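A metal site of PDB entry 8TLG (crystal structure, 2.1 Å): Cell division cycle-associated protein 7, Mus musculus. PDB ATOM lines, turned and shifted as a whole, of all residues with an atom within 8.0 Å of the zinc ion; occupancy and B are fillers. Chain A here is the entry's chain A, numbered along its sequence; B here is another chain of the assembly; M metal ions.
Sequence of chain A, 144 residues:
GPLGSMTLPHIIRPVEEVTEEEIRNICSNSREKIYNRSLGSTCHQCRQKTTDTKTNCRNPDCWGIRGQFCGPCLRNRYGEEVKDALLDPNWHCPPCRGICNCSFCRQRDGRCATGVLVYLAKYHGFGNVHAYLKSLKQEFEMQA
Merely in contact with the zinc ion: Lys 33. Five residues have an atom within 4 Å of the zinc ion: Lys 33, Cys 43, Cys 46, Cys 70 and Cys 73. The nearest printed residue that does not touch the zinc ion is Gln 45 (4.4 Å).
The side-chain sulfur of Cys 46 lies close to the side-chain amino group of Lys 33, at 3.3 Å. The side-chain amide nitrogen (NE2) of Gln 48 is in hydrogen-bond range of the backbone carbonyl oxygen (O) of Cys 46. The side-chain sulfur of Cys 70 sits close to the side-chain amino group of Lys 33. N of Gln 45 sits close to SG of Cys 43, at 3.4 Å. O of Gln 48 lies within hydrogen-bond range of N of Cys 43, 3.1 Å away.
The zinc ion is bound by SG of Cys 46 (2.2 Å), SG of Cys 70 (2.3 Å), SG of Cys 43 (2.3 Å) and SG of Cys 73 (2.3 Å).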
ATOM      1  N   CYS A  27       1.007 -26.581   4.421  1.00  0.00           N
ATOM      2  CA  CYS A  27       0.210 -25.672   5.236  1.00  0.00           C
ATOM      3  C   CYS A  27      -1.094 -25.315   4.520  1.00  0.00           C
ATOM      4  O   CYS A  27      -1.088 -24.930   3.350  1.00  0.00           O
ATOM      5  CB  CYS A  27       0.996 -24.416   5.563  1.00  0.00           C
ATOM      6  SG  CYS A  27       0.052 -23.205   6.502  1.00  0.00           S
ATOM      7  N   SER A  30      -2.307 -19.983   7.106  1.00  0.00           N
ATOM      8  CA  SER A  30      -1.092 -19.314   7.588  1.00  0.00           C
ATOM      9  C   SER A  30      -0.998 -19.307   9.109  1.00  0.00           C
ATOM     10  O   SER A  30       0.104 -19.365   9.660  1.00  0.00           O
ATOM     11  CB  SER A  30      -1.027 -17.887   7.054  1.00  0.00           C
ATOM     12  OG  SER A  30       0.047 -17.197   7.648  1.00  0.00           O
ATOM     13  N   LYS A  33       0.737 -22.471  11.302  1.00  0.00           N
ATOM     14  CA  LYS A  33       2.129 -22.840  11.137  1.00  0.00           C
ATOM     15  C   LYS A  33       2.818 -23.088  12.474  1.00  0.00           C
ATOM     16  O   LYS A  33       2.466 -22.488  13.497  1.00  0.00           O
ATOM     17  CB  LYS A  33       2.881 -21.753  10.367  1.00  0.00           C
ATOM     18  CG  LYS A  33       2.479 -21.632   8.918  1.00  0.00           C
ATOM     19  CD  LYS A  33       3.329 -20.591   8.210  1.00  0.00           C
ATOM     20  CE  LYS A  33       2.988 -20.520   6.722  1.00  0.00           C
ATOM     21  NZ  LYS A  33       3.772 -19.464   6.032  1.00  0.00           N
ATOM     22  N   SER A  41      11.753 -24.398   7.764  1.00  0.00           N
ATOM     23  CA  SER A  41      12.211 -23.903   6.469  1.00  0.00           C
ATOM     24  C   SER A  41      11.526 -22.575   6.190  1.00  0.00           C
ATOM     25  O   SER A  41      10.341 -22.402   6.469  1.00  0.00           O
ATOM     26  CB  SER A  41      11.900 -24.902   5.346  1.00  0.00           C
ATOM     27  OG  SER A  41      10.522 -25.239   5.345  1.00  0.00           O
ATOM     28  N   THR A  42      12.289 -21.631   5.643  1.00  0.00           N
ATOM     29  CA  THR A  42      11.790 -20.283   5.390  1.00  0.00           C
ATOM     30  C   THR A  42      11.070 -20.230   4.053  1.00  0.00           C
ATOM     31  O   THR A  42      11.595 -20.696   3.036  1.00  0.00           O
ATOM     32  CB  THR A  42      12.939 -19.278   5.401  1.00  0.00           C
ATOM     33  OG1 THR A  42      13.564 -19.290   6.682  1.00  0.00           O
ATOM     34  CG2 THR A  42      12.419 -17.885   5.084  1.00  0.00           C
ATOM     35  N   CYS A  43       9.860 -19.660   4.054  1.00  0.00           N
ATOM     36  CA  CYS A  43       9.165 -19.349   2.817  1.00  0.00           C
ATOM     37  C   CYS A  43       9.711 -18.039   2.263  1.00  0.00           C
ATOM     38  O   CYS A  43       9.771 -17.033   2.979  1.00  0.00           O
ATOM     39  CB  CYS A  43       7.659 -19.257   3.057  1.00  0.00           C
ATOM     40  SG  CYS A  43       6.703 -18.631   1.655  1.00  0.00           S
ATOM     41  N   HIS A  44      10.107 -18.046   0.983  1.00  0.00           N
ATOM     42  CA  HIS A  44      10.667 -16.833   0.394  1.00  0.00           C
ATOM     43  C   HIS A  44       9.660 -15.693   0.384  1.00  0.00           C
ATOM     44  O   HIS A  44      10.042 -14.525   0.550  1.00  0.00           O
ATOM     45  CB  HIS A  44      11.140 -17.118  -1.037  1.00  0.00           C
ATOM     46  CG  HIS A  44      11.506 -15.895  -1.810  1.00  0.00           C
ATOM     47  ND1 HIS A  44      12.683 -15.198  -1.604  1.00  0.00           N
ATOM     48  CD2 HIS A  44      10.843 -15.230  -2.793  1.00  0.00           C
ATOM     49  CE1 HIS A  44      12.730 -14.162  -2.425  1.00  0.00           C
ATOM     50  NE2 HIS A  44      11.630 -14.156  -3.157  1.00  0.00           N
ATOM     51  N   GLN A  45       8.373 -16.000   0.227  1.00  0.00           N
ATOM     52  CA  GLN A  45       7.371 -14.952   0.072  1.00  0.00           C
ATOM     53  C   GLN A  45       7.093 -14.263   1.408  1.00  0.00           C
ATOM     54  O   GLN A  45       7.261 -13.044   1.533  1.00  0.00           O
ATOM     55  CB  GLN A  45       6.088 -15.537  -0.516  1.00  0.00           C
ATOM     56  CG  GLN A  45       5.035 -14.502  -0.879  1.00  0.00           C
ATOM     57  CD  GLN A  45       5.323 -13.826  -2.212  1.00  0.00           C
ATOM     58  OE1 GLN A  45       6.079 -14.341  -3.037  1.00  0.00           O
ATOM     59  NE2 GLN A  45       4.703 -12.672  -2.433  1.00  0.00           N
ATOM     60  N   CYS A  46       6.673 -15.020   2.423  1.00  0.00           N
ATOM     61  CA  CYS A  46       6.299 -14.443   3.704  1.00  0.00           C
ATOM     62  C   CYS A  46       7.443 -14.421   4.723  1.00  0.00           C
ATOM     63  O   CYS A  46       7.280 -13.828   5.791  1.00  0.00           O
ATOM     64  CB  CYS A  46       5.111 -15.192   4.296  1.00  0.00           C
ATOM     65  SG  CYS A  46       5.414 -16.918   4.677  1.00  0.00           S
ATOM     66  N   ARG A  47       8.574 -15.059   4.413  1.00  0.00           N
ATOM     67  CA  ARG A  47       9.790 -14.966   5.220  1.00  0.00           C
ATOM     68  C   ARG A  47       9.598 -15.505   6.640  1.00  0.00           C
ATOM     69  O   ARG A  47      10.218 -15.026   7.591  1.00  0.00           O
ATOM     70  CB  ARG A  47      10.327 -13.537   5.239  1.00  0.00           C
ATOM     71  CG  ARG A  47      10.560 -12.972   3.843  1.00  0.00           C
ATOM     72  CD  ARG A  47      11.344 -11.672   3.846  1.00  0.00           C
ATOM     73  NE  ARG A  47      10.534 -10.515   4.234  1.00  0.00           N
ATOM     74  CZ  ARG A  47       9.819  -9.785   3.388  1.00  0.00           C
ATOM     75  NH1 ARG A  47       9.748 -10.090   2.097  1.00  0.00           N
ATOM     76  NH2 ARG A  47       9.170  -8.728   3.837  1.00  0.00           N
ATOM     77  N   GLN A  48       8.731 -16.514   6.787  1.00  0.00           N
ATOM     78  CA  GLN A  48       8.529 -17.204   8.054  1.00  0.00           C
ATOM     79  C   GLN A  48       9.194 -18.572   8.000  1.00  0.00           C
ATOM     80  O   GLN A  48       9.000 -19.318   7.032  1.00  0.00           O
ATOM     81  CB  GLN A  48       7.039 -17.347   8.375  1.00  0.00           C
ATOM     82  CG  GLN A  48       6.244 -16.051   8.299  1.00  0.00           C
ATOM     83  CD  GLN A  48       6.765 -14.980   9.235  1.00  0.00           C
ATOM     84  OE1 GLN A  48       6.626 -15.097  10.459  1.00  0.00           O
ATOM     85  NE2 GLN A  48       7.361 -13.941   8.681  1.00  0.00           N
ATOM     86  N   THR A  50       9.175 -22.087   9.241  1.00  0.00           N
ATOM     87  CA  THR A  50       8.222 -22.995   9.855  1.00  0.00           C
ATOM     88  C   THR A  50       8.425 -24.395   9.289  1.00  0.00           C
ATOM     89  O   THR A  50       9.132 -24.584   8.292  1.00  0.00           O
ATOM     90  CB  THR A  50       6.782 -22.523   9.642  1.00  0.00           C
ATOM     91  OG1 THR A  50       6.530 -22.362   8.236  1.00  0.00           O
ATOM     92  CG2 THR A  50       6.535 -21.186  10.331  1.00  0.00           C
ATOM     93  N   ASP A  52       6.142 -26.562   8.047  1.00  0.00           N
ATOM     94  CA  ASP A  52       5.269 -27.071   7.004  1.00  0.00           C
ATOM     95  C   ASP A  52       6.037 -27.238   5.690  1.00  0.00           C
ATOM     96  O   ASP A  52       7.047 -26.569   5.435  1.00  0.00           O
ATOM     97  CB  ASP A  52       4.071 -26.156   6.804  1.00  0.00           C
ATOM     98  CG  ASP A  52       4.467 -24.690   6.748  1.00  0.00           C
ATOM     99  OD1 ASP A  52       4.940 -24.174   7.772  1.00  0.00           O
ATOM    100  OD2 ASP A  52       4.328 -24.067   5.670  1.00  0.00           O
ATOM    101  N   LYS A  54       7.382 -26.962   2.093  1.00  0.00           N
ATOM    102  CA  LYS A  54       7.541 -25.913   1.094  1.00  0.00           C
ATOM    103  C   LYS A  54       7.797 -26.530  -0.274  1.00  0.00           C
ATOM    104  O   LYS A  54       8.054 -27.728  -0.413  1.00  0.00           O
ATOM    105  CB  LYS A  54       8.685 -24.965   1.462  1.00  0.00           C
ATOM    106  CG  LYS A  54       8.726 -24.516   2.907  1.00  0.00           C
ATOM    107  CD  LYS A  54       7.496 -23.723   3.294  1.00  0.00           C
ATOM    108  CE  LYS A  54       7.715 -23.001   4.614  1.00  0.00           C
ATOM    109  NZ  LYS A  54       8.148 -23.931   5.701  1.00  0.00           N
ATOM    110  N   GLN A  68      11.656 -21.747  -2.119  1.00  0.00           N
ATOM    111  CA  GLN A  68      10.821 -22.381  -1.113  1.00  0.00           C
ATOM    112  C   GLN A  68       9.622 -21.497  -0.823  1.00  0.00           C
ATOM    113  O   GLN A  68       9.783 -20.368  -0.349  1.00  0.00           O
ATOM    114  CB  GLN A  68      11.621 -22.646   0.169  1.00  0.00           C
ATOM    115  CG  GLN A  68      12.854 -23.508  -0.044  1.00  0.00           C
ATOM    116  CD  GLN A  68      13.664 -23.657   1.220  1.00  0.00           C
ATOM    117  OE1 GLN A  68      13.340 -23.091   2.259  1.00  0.00           O
ATOM    118  NE2 GLN A  68      14.738 -24.434   1.132  1.00  0.00           N
ATOM    119  N   PHE A  69       8.426 -22.018  -1.081  1.00  0.00           N
ATOM    120  CA  PHE A  69       7.182 -21.291  -0.876  1.00  0.00           C
ATOM    121  C   PHE A  69       6.214 -22.146  -0.086  1.00  0.00           C
ATOM    122  O   PHE A  69       6.080 -23.346  -0.346  1.00  0.00           O
ATOM    123  CB  PHE A  69       6.554 -20.877  -2.220  1.00  0.00           C
ATOM    124  CG  PHE A  69       7.296 -19.769  -2.920  1.00  0.00           C
ATOM    125  CD1 PHE A  69       8.482 -20.029  -3.601  1.00  0.00           C
ATOM    126  CD2 PHE A  69       6.822 -18.469  -2.890  1.00  0.00           C
ATOM    127  CE1 PHE A  69       9.166 -19.018  -4.233  1.00  0.00           C
ATOM    128  CE2 PHE A  69       7.503 -17.453  -3.530  1.00  0.00           C
ATOM    129  CZ  PHE A  69       8.674 -17.724  -4.198  1.00  0.00           C
ATOM    130  N   CYS A  70       5.535 -21.532   0.873  1.00  0.00           N
ATOM    131  CA  CYS A  70       4.575 -22.258   1.695  1.00  0.00           C
ATOM    132  C   CYS A  70       3.269 -22.450   0.918  1.00  0.00           C
ATOM    133  O   CYS A  70       3.039 -21.866  -0.142  1.00  0.00           O
ATOM    134  CB  CYS A  70       4.320 -21.526   3.011  1.00  0.00           C
ATOM    135  SG  CYS A  70       3.449 -19.941   2.858  1.00  0.00           S
ATOM    136  N   GLY A  71       2.402 -23.302   1.474  1.00  0.00           N
ATOM    137  CA  GLY A  71       1.100 -23.565   0.908  1.00  0.00           C
ATOM    138  C   GLY A  71       0.308 -22.309   0.620  1.00  0.00           C
ATOM    139  O   GLY A  71      -0.040 -22.025  -0.534  1.00  0.00           O
ATOM    140  N   PRO A  72      -0.019 -21.545   1.665  1.00  0.00           N
ATOM    141  CA  PRO A  72      -0.826 -20.326   1.438  1.00  0.00           C
ATOM    142  C   PRO A  72      -0.177 -19.319   0.505  1.00  0.00           C
ATOM    143  O   PRO A  72      -0.892 -18.664  -0.275  1.00  0.00           O
ATOM    144  CB  PRO A  72      -0.996 -19.761   2.858  1.00  0.00           C
ATOM    145  CG  PRO A  72      -0.843 -20.940   3.755  1.00  0.00           C
ATOM    146  CD  PRO A  72       0.189 -21.810   3.099  1.00  0.00           C
ATOM    147  N   CYS A  73       1.140 -19.152   0.552  1.00  0.00           N
ATOM    148  CA  CYS A  73       1.781 -18.110  -0.247  1.00  0.00           C
ATOM    149  C   CYS A  73       1.758 -18.451  -1.732  1.00  0.00           C
ATOM    150  O   CYS A  73       1.437 -17.593  -2.570  1.00  0.00           O
ATOM    151  CB  CYS A  73       3.216 -17.890   0.235  1.00  0.00           C
ATOM    152  SG  CYS A  73       3.349 -16.702   1.591  1.00  0.00           S
ATOM    153  N   LEU A  74       2.090 -19.693  -2.097  1.00  0.00           N
ATOM    154  CA  LEU A  74       1.991 -20.090  -3.489  1.00  0.00           C
ATOM    155  C   LEU A  74       0.537 -20.086  -3.953  1.00  0.00           C
ATOM    156  O   LEU A  74       0.235 -19.738  -5.099  1.00  0.00           O
ATOM    157  CB  LEU A  74       2.608 -21.472  -3.700  1.00  0.00           C
ATOM    158  CG  LEU A  74       2.942 -21.811  -5.152  1.00  0.00           C
ATOM    159  CD1 LEU A  74       4.152 -20.993  -5.615  1.00  0.00           C
ATOM    160  CD2 LEU A  74       3.191 -23.298  -5.329  1.00  0.00           C
ATOM    161  N   ARG A  77      -0.460 -15.968  -3.836  1.00  0.00           N
ATOM    162  CA  ARG A  77       0.326 -15.020  -4.615  1.00  0.00           C
ATOM    163  C   ARG A  77       0.556 -15.459  -6.057  1.00  0.00           C
ATOM    164  O   ARG A  77       0.947 -14.627  -6.876  1.00  0.00           O
ATOM    165  CB  ARG A  77       1.672 -14.765  -3.932  1.00  0.00           C
ATOM    166  CG  ARG A  77       1.568 -14.360  -2.471  1.00  0.00           C
ATOM    167  CD  ARG A  77       0.882 -13.010  -2.314  1.00  0.00           C
ATOM    168  NE  ARG A  77       1.680 -11.926  -2.874  1.00  0.00           N
ATOM    169  CZ  ARG A  77       1.468 -10.641  -2.657  1.00  0.00           C
ATOM    170  NH1 ARG A  77       0.472 -10.231  -1.889  1.00  0.00           N
ATOM    171  NH2 ARG A  77       2.258  -9.736  -3.231  1.00  0.00           N
ATOM    172  P    DG B  11      -4.307 -17.685   4.554  1.00  0.00           P
ATOM    173  OP1  DG B  11      -4.221 -18.150   3.154  1.00  0.00           O
ATOM    174  OP2  DG B  11      -3.801 -18.541   5.642  1.00  0.00           O
ATOM    175  O5'  DG B  11      -3.589 -16.258   4.678  1.00  0.00           O
ATOM    176  C5'  DG B  11      -2.608 -15.853   3.717  1.00  0.00           C
ATOM    177  C4'  DG B  11      -3.113 -14.695   2.863  1.00  0.00           C
ATOM    178  O4'  DG B  11      -4.521 -14.455   3.129  1.00  0.00           O
ATOM    179  C3'  DG B  11      -2.421 -13.354   3.111  1.00  0.00           C
ATOM    180  O3'  DG B  11      -2.409 -12.607   1.899  1.00  0.00           O
ATOM    181  C2'  DG B  11      -3.335 -12.699   4.138  1.00  0.00           C
ATOM    182  C1'  DG B  11      -4.704 -13.154   3.644  1.00  0.00           C
ATOM    183  N9   DG B  11      -5.713 -13.216   4.698  1.00  0.00           N
ATOM    184  C8   DG B  11      -5.494 -13.297   6.043  1.00  0.00           C
ATOM    185  N7   DG B  11      -6.585 -13.357   6.746  1.00  0.00           N
ATOM    186  C5   DG B  11      -7.606 -13.302   5.798  1.00  0.00           C
ATOM    187  C6   DG B  11      -9.005 -13.331   5.954  1.00  0.00           C
ATOM    188  O6   DG B  11      -9.663 -13.398   7.013  1.00  0.00           O
ATOM    189  N1   DG B  11      -9.668 -13.258   4.734  1.00  0.00           N
ATOM    190  C2   DG B  11      -9.048 -13.181   3.504  1.00  0.00           C
ATOM    191  N2   DG B  11      -9.852 -13.119   2.439  1.00  0.00           N
ATOM    192  N3   DG B  11      -7.734 -13.161   3.345  1.00  0.00           N
ATOM    193  C4   DG B  11      -7.076 -13.219   4.526  1.00  0.00           C
ATOM    194  P    DT B  12      -1.022 -12.344   1.135  1.00  0.00           P
ATOM    195  OP1  DT B  12      -1.337 -11.586  -0.103  1.00  0.00           O
ATOM    196  OP2  DT B  12      -0.298 -13.626   1.046  1.00  0.00           O
ATOM    197  O5'  DT B  12      -0.209 -11.385   2.124  1.00  0.00           O
ATOM    198  C5'  DT B  12      -0.614 -10.040   2.307  1.00  0.00           C
ATOM    199  C4'  DT B  12       0.388  -9.292   3.160  1.00  0.00           C
ATOM    200  O4'  DT B  12       0.400  -9.865   4.481  1.00  0.00           O
ATOM    201  C3'  DT B  12       1.828  -9.369   2.688  1.00  0.00           C
ATOM    202  O3'  DT B  12       2.084  -8.311   1.778  1.00  0.00           O
ATOM    203  C2'  DT B  12       2.633  -9.206   3.973  1.00  0.00           C
ATOM    204  C1'  DT B  12       1.686  -9.705   5.063  1.00  0.00           C
ATOM    205  N1   DT B  12       2.092 -11.002   5.648  1.00  0.00           N
ATOM    206  C2   DT B  12       2.999 -11.005   6.688  1.00  0.00           C
ATOM    207  O2   DT B  12       3.489  -9.998   7.136  1.00  0.00           O
ATOM    208  N3   DT B  12       3.307 -12.253   7.172  1.00  0.00           N
ATOM    209  C4   DT B  12       2.802 -13.462   6.737  1.00  0.00           C
ATOM    210  O4   DT B  12       3.139 -14.529   7.239  1.00  0.00           O
ATOM    211  C5   DT B  12       1.857 -13.388   5.646  1.00  0.00           C
ATOM    212  C7   DT B  12       1.238 -14.639   5.095  1.00  0.00           C
ATOM    213  C6   DT B  12       1.541 -12.173   5.170  1.00  0.00           C
HETATM  214 ZN    ZN M   1       4.783 -18.062   2.852  1.00  0.00          ZN
